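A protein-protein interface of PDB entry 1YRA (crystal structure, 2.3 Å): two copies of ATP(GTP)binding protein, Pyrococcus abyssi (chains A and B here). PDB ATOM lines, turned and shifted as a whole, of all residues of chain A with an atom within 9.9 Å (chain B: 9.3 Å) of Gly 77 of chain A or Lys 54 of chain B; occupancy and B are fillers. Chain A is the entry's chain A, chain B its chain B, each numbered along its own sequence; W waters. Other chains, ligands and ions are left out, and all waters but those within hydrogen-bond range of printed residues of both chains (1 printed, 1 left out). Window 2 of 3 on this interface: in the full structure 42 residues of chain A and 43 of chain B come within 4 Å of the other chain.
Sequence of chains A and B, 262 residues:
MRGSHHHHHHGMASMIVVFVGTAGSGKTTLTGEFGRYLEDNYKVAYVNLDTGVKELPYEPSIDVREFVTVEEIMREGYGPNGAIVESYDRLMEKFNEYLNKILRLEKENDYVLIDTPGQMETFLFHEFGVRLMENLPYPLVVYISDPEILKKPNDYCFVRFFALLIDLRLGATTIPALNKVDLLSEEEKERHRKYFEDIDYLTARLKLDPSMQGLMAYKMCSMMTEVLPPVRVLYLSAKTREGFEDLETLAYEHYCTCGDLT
The side-chain amino group (NZ) of Lys 54 of chain B lies within hydrogen-bond range of the backbone carbonyl oxygen (O) of Gly 77 of chain A (2.8 Å).
The backbone NH (N) of Asp 50 of chain B sits close to the side-chain amide nitrogen (ND2) of Asn 48 of chain B, at 3.0 Å. OD1 of Asp 50 of chain B is in hydrogen-bond range of N of Gly 52 of chain B (3.0 Å). The backbone NH (N) of Val 70 of chain B sits at hydrogen-bond distance from the backbone carbonyl oxygen (O) of Thr 51 of chain B (2.9 Å). The guanidinium group (NH1) of Arg 65 of chain B lies within hydrogen-bond range of the backbone carbonyl oxygen (O) of Lys 54 of chain B, at 3.1 Å.
Pro 80 of chain A touches Gly 52 of chain B. Pro 80 of chain A touches Val 70 of chain B (CG to CG1, 3.7 Å). Glu 71 of chain B touches Pro 80 of chain A (OE2 to CD, 3.5 Å). Asn 81 of chain A touches Asp 50 of chain B.
Gly 77 of chain A touches just one residue of chain B: Lys 54. Lys 54 of chain B touches just one residue of chain A: Gly 77 (2.8 Å). Printed residues of chain B within 4 Å of Asn 81 of chain A: Asp 50 (3.6 Å). Of the printed residues of chain A, Gly 52 of chain B touches Pro 80 (3.5 Å). Printed residues of chain A within 4 Å of Glu 71 of chain B: Pro 80 (3.5 Å). Of the printed residues of chain A, Asp 50 of chain B touches Asn 81 (3.6 Å). The nearest printed residue of chain B that does not touch Gly 77 of chain A is Glu 71 of chain B (7.6 Å). The nearest residue of chain A that does not touch Lys 54 of chain B is Gly 79 of chain A (4.2 Å).
Printed residues of chain B that touch a printed residue of chain A: Asp 50, Gly 52, Lys 54, Val 70 and Glu 71. Hydrophobic or aromatic side chains of chain B within 4 Å of the printed part of chain A: Val 70. Along chain B the printed residues that touch a printed residue of chain A span positions 50 to 71. Hydrophobic or aromatic side chains of chain A that line the printed part of chain B: Pro 80. Among the printed residues, 5 pairs touch across the chains.
Positions printed for both chains: 70, 71 and 75. Of the 5 pairs that touch across the chains among the printed residues, none has its exchanged pair printed and touching as well.
Water W1 lies within hydrogen-bond range of OD1 of Asp 50 of chain B, ND2 of Asn 81 of chain A and OG1 of Thr 51 of chain B.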
ATOM      1  N   VAL A  70      15.997  18.346 -10.488  1.00  0.00           N
ATOM      2  CA  VAL A  70      15.269  19.560 -10.140  1.00  0.00           C
ATOM      3  C   VAL A  70      14.618  19.415  -8.758  1.00  0.00           C
ATOM      4  O   VAL A  70      14.646  20.346  -7.952  1.00  0.00           O
ATOM      5  CB  VAL A  70      14.200  19.847 -11.205  1.00  0.00           C
ATOM      6  CG1 VAL A  70      13.188  20.856 -10.702  1.00  0.00           C
ATOM      7  CG2 VAL A  70      14.865  20.309 -12.508  1.00  0.00           C
ATOM      8  N   GLU A  71      14.044  18.240  -8.486  1.00  0.00           N
ATOM      9  CA  GLU A  71      13.361  17.989  -7.212  1.00  0.00           C
ATOM     10  C   GLU A  71      14.317  18.140  -6.042  1.00  0.00           C
ATOM     11  O   GLU A  71      13.979  18.760  -5.033  1.00  0.00           O
ATOM     12  CB  GLU A  71      12.744  16.595  -7.191  1.00  0.00           C
ATOM     13  CG  GLU A  71      11.514  16.437  -8.087  1.00  0.00           C
ATOM     14  CD  GLU A  71      11.873  16.187  -9.550  1.00  0.00           C
ATOM     15  OE1 GLU A  71      12.985  16.578  -9.982  1.00  0.00           O
ATOM     16  OE2 GLU A  71      11.037  15.581 -10.263  1.00  0.00           O
ATOM     17  N   GLU A  72      15.514  17.582  -6.198  1.00  0.00           N
ATOM     18  CA  GLU A  72      16.560  17.660  -5.193  1.00  0.00           C
ATOM     19  C   GLU A  72      16.903  19.120  -4.911  1.00  0.00           C
ATOM     20  O   GLU A  72      17.033  19.545  -3.754  1.00  0.00           O
ATOM     21  CB  GLU A  72      17.792  16.889  -5.677  1.00  0.00           C
ATOM     22  CG  GLU A  72      18.997  16.975  -4.764  1.00  0.00           C
ATOM     23  CD  GLU A  72      18.824  16.228  -3.421  1.00  0.00           C
ATOM     24  OE1 GLU A  72      19.659  16.491  -2.519  1.00  0.00           O
ATOM     25  OE2 GLU A  72      17.896  15.384  -3.267  1.00  0.00           O
ATOM     26  N   ILE A  73      17.010  19.906  -5.976  1.00  0.00           N
ATOM     27  CA  ILE A  73      17.379  21.300  -5.817  1.00  0.00           C
ATOM     28  C   ILE A  73      16.268  22.097  -5.145  1.00  0.00           C
ATOM     29  O   ILE A  73      16.531  22.974  -4.313  1.00  0.00           O
ATOM     30  CB  ILE A  73      17.822  21.904  -7.164  1.00  0.00           C
ATOM     31  CG1 ILE A  73      19.048  21.117  -7.671  1.00  0.00           C
ATOM     32  CG2 ILE A  73      18.109  23.387  -7.027  1.00  0.00           C
ATOM     33  CD1 ILE A  73      19.623  21.615  -8.994  1.00  0.00           C
ATOM     34  N   MET A  74      15.025  21.799  -5.496  1.00  0.00           N
ATOM     35  CA  MET A  74      13.894  22.465  -4.854  1.00  0.00           C
ATOM     36  C   MET A  74      13.875  22.173  -3.352  1.00  0.00           C
ATOM     37  O   MET A  74      13.369  22.974  -2.589  1.00  0.00           O
ATOM     38  CB  MET A  74      12.570  22.035  -5.486  1.00  0.00           C
ATOM     39  CG  MET A  74      12.309  22.599  -6.884  1.00  0.00           C
ATOM     40  SD  MET A  74      10.902  21.796  -7.649  1.00  0.00           S
ATOM     41  CE  MET A  74       9.583  22.250  -6.517  1.00  0.00           C
ATOM     42  N   ARG A  75      14.426  21.030  -2.933  1.00  0.00           N
ATOM     43  CA  ARG A  75      14.511  20.712  -1.505  1.00  0.00           C
ATOM     44  C   ARG A  75      15.373  21.729  -0.806  1.00  0.00           C
ATOM     45  O   ARG A  75      15.180  21.986   0.368  1.00  0.00           O
ATOM     46  CB  ARG A  75      15.080  19.311  -1.226  1.00  0.00           C
ATOM     47  CG  ARG A  75      14.596  18.229  -2.165  1.00  0.00           C
ATOM     48  CD  ARG A  75      14.107  16.984  -1.435  1.00  0.00           C
ATOM     49  NE  ARG A  75      12.652  16.883  -1.553  1.00  0.00           N
ATOM     50  CZ  ARG A  75      12.014  16.268  -2.552  1.00  0.00           C
ATOM     51  NH1 ARG A  75      12.706  15.674  -3.526  1.00  0.00           N
ATOM     52  NH2 ARG A  75      10.683  16.224  -2.572  1.00  0.00           N
ATOM     53  N   GLU A  76      16.329  22.304  -1.528  1.00  0.00           N
ATOM     54  CA  GLU A  76      17.170  23.365  -0.993  1.00  0.00           C
ATOM     55  C   GLU A  76      16.439  24.700  -0.960  1.00  0.00           C
ATOM     56  O   GLU A  76      17.062  25.746  -0.782  1.00  0.00           O
ATOM     57  CB  GLU A  76      18.437  23.517  -1.839  1.00  0.00           C
ATOM     58  CG  GLU A  76      19.346  22.315  -1.836  1.00  0.00           C
ATOM     59  CD  GLU A  76      20.465  22.434  -2.849  1.00  0.00           C
ATOM     60  OE1 GLU A  76      20.791  23.584  -3.230  1.00  0.00           O
ATOM     61  OE2 GLU A  76      21.024  21.385  -3.260  1.00  0.00           O
ATOM     62  N   GLY A  77      15.129  24.688  -1.170  1.00  0.00           N
ATOM     63  CA  GLY A  77      14.356  25.915  -1.067  1.00  0.00           C
ATOM     64  C   GLY A  77      14.195  26.746  -2.328  1.00  0.00           C
ATOM     65  O   GLY A  77      13.541  27.797  -2.308  1.00  0.00           O
ATOM     66  N   TYR A  78      14.796  26.293  -3.424  1.00  0.00           N
ATOM     67  CA  TYR A  78      14.573  26.911  -4.748  1.00  0.00           C
ATOM     68  C   TYR A  78      13.152  26.656  -5.230  1.00  0.00           C
ATOM     69  O   TYR A  78      12.588  25.607  -4.966  1.00  0.00           O
ATOM     70  CB  TYR A  78      15.497  26.278  -5.788  1.00  0.00           C
ATOM     71  CG  TYR A  78      16.922  26.698  -5.737  1.00  0.00           C
ATOM     72  CD1 TYR A  78      17.362  27.779  -6.469  1.00  0.00           C
ATOM     73  CD2 TYR A  78      17.842  26.003  -4.974  1.00  0.00           C
ATOM     74  CE1 TYR A  78      18.662  28.160  -6.447  1.00  0.00           C
ATOM     75  CE2 TYR A  78      19.149  26.380  -4.942  1.00  0.00           C
ATOM     76  CZ  TYR A  78      19.552  27.471  -5.690  1.00  0.00           C
ATOM     77  OH  TYR A  78      20.861  27.879  -5.682  1.00  0.00           O
ATOM     78  N   GLY A  79      12.589  27.595  -5.974  1.00  0.00           N
ATOM     79  CA  GLY A  79      11.366  27.325  -6.716  1.00  0.00           C
ATOM     80  C   GLY A  79      11.681  26.450  -7.918  1.00  0.00           C
ATOM     81  O   GLY A  79      12.868  26.280  -8.296  1.00  0.00           O
ATOM     82  N   PRO A  80      10.637  25.854  -8.515  1.00  0.00           N
ATOM     83  CA  PRO A  80      10.824  24.983  -9.673  1.00  0.00           C
ATOM     84  C   PRO A  80      11.599  25.624 -10.803  1.00  0.00           C
ATOM     85  O   PRO A  80      12.546  25.026 -11.294  1.00  0.00           O
ATOM     86  CB  PRO A  80       9.395  24.643 -10.121  1.00  0.00           C
ATOM     87  CG  PRO A  80       8.473  25.481  -9.266  1.00  0.00           C
ATOM     88  CD  PRO A  80       9.230  25.910  -8.069  1.00  0.00           C
ATOM     89  N   ASN A  81      11.218  26.822 -11.230  1.00  0.00           N
ATOM     90  CA  ASN A  81      11.870  27.385 -12.405  1.00  0.00           C
ATOM     91  C   ASN A  81      13.285  27.772 -12.054  1.00  0.00           C
ATOM     92  O   ASN A  81      14.174  27.711 -12.897  1.00  0.00           O
ATOM     93  CB  ASN A  81      11.091  28.579 -12.986  1.00  0.00           C
ATOM     94  CG  ASN A  81       9.800  28.162 -13.639  1.00  0.00           C
ATOM     95  OD1 ASN A  81       9.787  27.247 -14.465  1.00  0.00           O
ATOM     96  ND2 ASN A  81       8.696  28.813 -13.270  1.00  0.00           N
ATOM     97  N   GLY A  82      13.492  28.173 -10.801  1.00  0.00           N
ATOM     98  CA  GLY A  82      14.839  28.493 -10.329  1.00  0.00           C
ATOM     99  C   GLY A  82      15.678  27.237 -10.241  1.00  0.00           C
ATOM    100  O   GLY A  82      16.873  27.253 -10.544  1.00  0.00           O
ATOM    101  N   ALA A  83      15.042  26.136  -9.856  1.00  0.00           N
ATOM    102  CA  ALA A  83      15.737  24.854  -9.666  1.00  0.00           C
ATOM    103  C   ALA A  83      16.159  24.314 -11.001  1.00  0.00           C
ATOM    104  O   ALA A  83      17.209  23.679 -11.118  1.00  0.00           O
ATOM    105  CB  ALA A  83      14.831  23.852  -8.945  1.00  0.00           C
ATOM    106  N   GLU A  86      19.190  26.403 -12.098  1.00  0.00           N
ATOM    107  CA  GLU A  86      20.263  26.095 -11.179  1.00  0.00           C
ATOM    108  C   GLU A  86      20.770  24.711 -11.510  1.00  0.00           C
ATOM    109  O   GLU A  86      21.969  24.457 -11.423  1.00  0.00           O
ATOM    110  CB  GLU A  86      19.756  26.177  -9.729  1.00  0.00           C
ATOM    111  CG  GLU A  86      20.716  25.667  -8.671  1.00  0.00           C
ATOM    112  CD  GLU A  86      21.960  26.517  -8.538  1.00  0.00           C
ATOM    113  OE1 GLU A  86      22.921  26.001  -7.943  1.00  0.00           O
ATOM    114  OE2 GLU A  86      21.987  27.681  -9.025  1.00  0.00           O
ATOM    115  N   ARG A  90      24.817  23.779 -12.324  1.00  0.00           N
ATOM    116  CA  ARG A  90      25.588  22.693 -11.700  1.00  0.00           C
ATOM    117  C   ARG A  90      26.115  21.659 -12.674  1.00  0.00           C
ATOM    118  O   ARG A  90      27.255  21.233 -12.543  1.00  0.00           O
ATOM    119  CB  ARG A  90      24.808  22.038 -10.566  1.00  0.00           C
ATOM    120  CG  ARG A  90      24.364  23.044  -9.514  1.00  0.00           C
ATOM    121  CD  ARG A  90      23.729  22.367  -8.307  1.00  0.00           C
ATOM    122  NE  ARG A  90      23.121  23.356  -7.444  1.00  0.00           N
ATOM    123  CZ  ARG A  90      22.572  23.093  -6.267  1.00  0.00           C
ATOM    124  NH1 ARG A  90      22.584  21.849  -5.800  1.00  0.00           N
ATOM    125  NH2 ARG A  90      22.010  24.076  -5.555  1.00  0.00           N
ATOM    126  N   THR B  28      11.077  38.900 -12.585  1.00  0.00           N
ATOM    127  CA  THR B  28      10.329  39.185 -11.374  1.00  0.00           C
ATOM    128  C   THR B  28      10.930  40.369 -10.621  1.00  0.00           C
ATOM    129  O   THR B  28      10.224  41.266 -10.164  1.00  0.00           O
ATOM    130  CB  THR B  28      10.194  37.904 -10.514  1.00  0.00           C
ATOM    131  OG1 THR B  28       9.203  37.051 -11.114  1.00  0.00           O
ATOM    132  CG2 THR B  28       9.779  38.235  -9.067  1.00  0.00           C
ATOM    133  N   ASN B  48       0.865  38.918 -11.522  1.00  0.00           N
ATOM    134  CA  ASN B  48       1.726  37.742 -11.613  1.00  0.00           C
ATOM    135  C   ASN B  48       1.013  36.591 -12.255  1.00  0.00           C
ATOM    136  O   ASN B  48       0.018  36.095 -11.727  1.00  0.00           O
ATOM    137  CB  ASN B  48       2.249  37.280 -10.266  1.00  0.00           C
ATOM    138  CG  ASN B  48       2.933  35.941 -10.365  1.00  0.00           C
ATOM    139  OD1 ASN B  48       2.560  34.972  -9.691  1.00  0.00           O
ATOM    140  ND2 ASN B  48       3.922  35.864 -11.230  1.00  0.00           N
ATOM    141  N   ASP B  50       2.816  33.854 -13.143  1.00  0.00           N
ATOM    142  CA  ASP B  50       3.779  32.740 -12.973  1.00  0.00           C
ATOM    143  C   ASP B  50       3.355  31.838 -11.815  1.00  0.00           C
ATOM    144  O   ASP B  50       3.418  32.237 -10.652  1.00  0.00           O
ATOM    145  CB  ASP B  50       5.164  33.326 -12.709  1.00  0.00           C
ATOM    146  CG  ASP B  50       6.249  32.286 -12.637  1.00  0.00           C
ATOM    147  OD1 ASP B  50       5.984  31.108 -12.955  1.00  0.00           O
ATOM    148  OD2 ASP B  50       7.391  32.678 -12.271  1.00  0.00           O
ATOM    149  N   THR B  51       2.929  30.626 -12.138  1.00  0.00           N
ATOM    150  CA  THR B  51       2.497  29.665 -11.116  1.00  0.00           C
ATOM    151  C   THR B  51       3.647  29.017 -10.374  1.00  0.00           C
ATOM    152  O   THR B  51       3.438  28.139  -9.531  1.00  0.00           O
ATOM    153  CB  THR B  51       1.695  28.516 -11.752  1.00  0.00           C
ATOM    154  OG1 THR B  51       2.461  27.953 -12.823  1.00  0.00           O
ATOM    155  CG2 THR B  51       0.374  29.006 -12.305  1.00  0.00           C
ATOM    156  N   GLY B  52       4.875  29.398 -10.694  1.00  0.00           N
ATOM    157  CA  GLY B  52       6.004  28.627 -10.176  1.00  0.00           C
ATOM    158  C   GLY B  52       7.038  29.454  -9.464  1.00  0.00           C
ATOM    159  O   GLY B  52       8.176  29.028  -9.295  1.00  0.00           O
ATOM    160  N   VAL B  53       6.651  30.655  -9.078  1.00  0.00           N
ATOM    161  CA  VAL B  53       7.560  31.569  -8.422  1.00  0.00           C
ATOM    162  C   VAL B  53       7.301  31.405  -6.942  1.00  0.00           C
ATOM    163  O   VAL B  53       6.156  31.209  -6.520  1.00  0.00           O
ATOM    164  CB  VAL B  53       7.296  33.026  -8.891  1.00  0.00           C
ATOM    165  CG1 VAL B  53       5.939  33.538  -8.371  1.00  0.00           C
ATOM    166  CG2 VAL B  53       8.468  33.973  -8.527  1.00  0.00           C
ATOM    167  N   LYS B  54       8.364  31.449  -6.151  1.00  0.00           N
ATOM    168  CA  LYS B  54       8.250  31.153  -4.729  1.00  0.00           C
ATOM    169  C   LYS B  54       7.866  32.392  -3.908  1.00  0.00           C
ATOM    170  O   LYS B  54       6.925  32.339  -3.119  1.00  0.00           O
ATOM    171  CB  LYS B  54       9.527  30.496  -4.202  1.00  0.00           C
ATOM    172  CG  LYS B  54       9.266  29.222  -3.394  1.00  0.00           C
ATOM    173  CD  LYS B  54      10.473  28.854  -2.523  1.00  0.00           C
ATOM    174  CE  LYS B  54      10.178  27.658  -1.631  1.00  0.00           C
ATOM    175  NZ  LYS B  54      11.315  27.372  -0.684  1.00  0.00           N
ATOM    176  N   GLU B  55       8.589  33.491  -4.083  1.00  0.00           N
ATOM    177  CA  GLU B  55       8.205  34.736  -3.429  1.00  0.00           C
ATOM    178  C   GLU B  55       8.203  35.939  -4.380  1.00  0.00           C
ATOM    179  O   GLU B  55       9.052  36.049  -5.254  1.00  0.00           O
ATOM    180  CB  GLU B  55       9.060  35.010  -2.173  1.00  0.00           C
ATOM    181  CG  GLU B  55      10.534  35.283  -2.433  1.00  0.00           C
ATOM    182  CD  GLU B  55      11.173  36.215  -1.380  1.00  0.00           C
ATOM    183  OE1 GLU B  55      10.441  36.798  -0.544  1.00  0.00           O
ATOM    184  OE2 GLU B  55      12.417  36.369  -1.397  1.00  0.00           O
ATOM    185  N   LEU B  56       7.239  36.837  -4.209  1.00  0.00           N
ATOM    186  CA  LEU B  56       7.179  38.064  -5.017  1.00  0.00           C
ATOM    187  C   LEU B  56       7.733  39.256  -4.257  1.00  0.00           C
ATOM    188  O   LEU B  56       7.412  39.450  -3.099  1.00  0.00           O
ATOM    189  CB  LEU B  56       5.744  38.367  -5.425  1.00  0.00           C
ATOM    190  CG  LEU B  56       5.054  37.301  -6.282  1.00  0.00           C
ATOM    191  CD1 LEU B  56       3.584  37.653  -6.473  1.00  0.00           C
ATOM    192  CD2 LEU B  56       5.775  37.125  -7.617  1.00  0.00           C
ATOM    193  N   PRO B  57       8.573  40.067  -4.919  1.00  0.00           N
ATOM    194  CA  PRO B  57       9.124  41.285  -4.327  1.00  0.00           C
ATOM    195  C   PRO B  57       8.119  42.431  -4.374  1.00  0.00           C
ATOM    196  O   PRO B  57       8.484  43.570  -4.098  1.00  0.00           O
ATOM    197  CB  PRO B  57      10.279  41.616  -5.254  1.00  0.00           C
ATOM    198  CG  PRO B  57       9.787  41.147  -6.598  1.00  0.00           C
ATOM    199  CD  PRO B  57       9.031  39.867  -6.305  1.00  0.00           C
ATOM    200  N   ASP B  63      -2.731  37.356  -8.786  1.00  0.00           N
ATOM    201  CA  ASP B  63      -1.728  36.322  -8.498  1.00  0.00           C
ATOM    202  C   ASP B  63      -2.319  34.965  -8.807  1.00  0.00           C
ATOM    203  O   ASP B  63      -3.091  34.427  -8.029  1.00  0.00           O
ATOM    204  CB  ASP B  63      -1.300  36.396  -7.032  1.00  0.00           C
ATOM    205  CG  ASP B  63      -0.086  35.539  -6.724  1.00  0.00           C
ATOM    206  OD1 ASP B  63       0.276  34.673  -7.559  1.00  0.00           O
ATOM    207  OD2 ASP B  63       0.515  35.730  -5.635  1.00  0.00           O
ATOM    208  N   ARG B  65      -1.137  32.206  -8.514  1.00  0.00           N
ATOM    209  CA  ARG B  65      -0.759  31.174  -7.503  1.00  0.00           C
ATOM    210  C   ARG B  65      -1.850  30.949  -6.468  1.00  0.00           C
ATOM    211  O   ARG B  65      -1.773  30.027  -5.647  1.00  0.00           O
ATOM    212  CB  ARG B  65       0.537  31.517  -6.764  1.00  0.00           C
ATOM    213  CG  ARG B  65       1.779  31.417  -7.623  1.00  0.00           C
ATOM    214  CD  ARG B  65       2.972  31.940  -6.875  1.00  0.00           C
ATOM    215  NE  ARG B  65       2.643  33.201  -6.243  1.00  0.00           N
ATOM    216  CZ  ARG B  65       3.316  33.712  -5.218  1.00  0.00           C
ATOM    217  NH1 ARG B  65       4.378  33.073  -4.749  1.00  0.00           N
ATOM    218  NH2 ARG B  65       2.920  34.853  -4.671  1.00  0.00           N
ATOM    219  N   THR B  69      -0.397  26.272  -7.837  1.00  0.00           N
ATOM    220  CA  THR B  69       1.063  26.384  -7.945  1.00  0.00           C
ATOM    221  C   THR B  69       1.652  25.146  -8.625  1.00  0.00           C
ATOM    222  O   THR B  69       1.072  24.082  -8.566  1.00  0.00           O
ATOM    223  CB  THR B  69       1.719  26.464  -6.563  1.00  0.00           C
ATOM    224  OG1 THR B  69       1.374  25.275  -5.824  1.00  0.00           O
ATOM    225  CG2 THR B  69       1.301  27.739  -5.793  1.00  0.00           C
ATOM    226  N   VAL B  70       2.816  25.293  -9.255  1.00  0.00           N
ATOM    227  CA  VAL B  70       3.573  24.164  -9.811  1.00  0.00           C
ATOM    228  C   VAL B  70       3.879  23.173  -8.692  1.00  0.00           C
ATOM    229  O   VAL B  70       3.822  21.944  -8.880  1.00  0.00           O
ATOM    230  CB  VAL B  70       4.896  24.626 -10.424  1.00  0.00           C
ATOM    231  CG1 VAL B  70       5.788  23.413 -10.789  1.00  0.00           C
ATOM    232  CG2 VAL B  70       4.640  25.520 -11.619  1.00  0.00           C
ATOM    233  N   GLU B  71       4.176  23.719  -7.519  1.00  0.00           N
ATOM    234  CA  GLU B  71       4.558  22.910  -6.373  1.00  0.00           C
ATOM    235  C   GLU B  71       3.415  22.017  -5.894  1.00  0.00           C
ATOM    236  O   GLU B  71       3.602  20.813  -5.719  1.00  0.00           O
ATOM    237  CB  GLU B  71       5.126  23.798  -5.256  1.00  0.00           C
ATOM    238  CG  GLU B  71       6.382  24.590  -5.691  1.00  0.00           C
ATOM    239  CD  GLU B  71       6.088  26.011  -6.185  1.00  0.00           C
ATOM    240  OE1 GLU B  71       5.186  26.183  -7.034  1.00  0.00           O
ATOM    241  OE2 GLU B  71       6.786  26.951  -5.722  1.00  0.00           O
ATOM    242  N   ARG B  75       3.147  17.693  -6.015  1.00  0.00           N
ATOM    243  CA  ARG B  75       2.655  16.826  -4.937  1.00  0.00           C
ATOM    244  C   ARG B  75       1.632  15.824  -5.444  1.00  0.00           C
ATOM    245  O   ARG B  75       1.341  14.856  -4.765  1.00  0.00           O
ATOM    246  CB  ARG B  75       2.023  17.639  -3.792  1.00  0.00           C
ATOM    247  CG  ARG B  75       2.966  18.643  -3.166  1.00  0.00           C
ATOM    248  CD  ARG B  75       2.434  19.189  -1.848  1.00  0.00           C
ATOM    249  NE  ARG B  75       3.288  20.277  -1.353  1.00  0.00           N
ATOM    250  CZ  ARG B  75       4.609  20.183  -1.169  1.00  0.00           C
ATOM    251  NH1 ARG B  75       5.249  19.055  -1.438  1.00  0.00           N
ATOM    252  NH2 ARG B  75       5.300  21.223  -0.715  1.00  0.00           N
HETATM  253  O   HOH W   1       5.565  28.787 -14.171  1.00  0.00           O
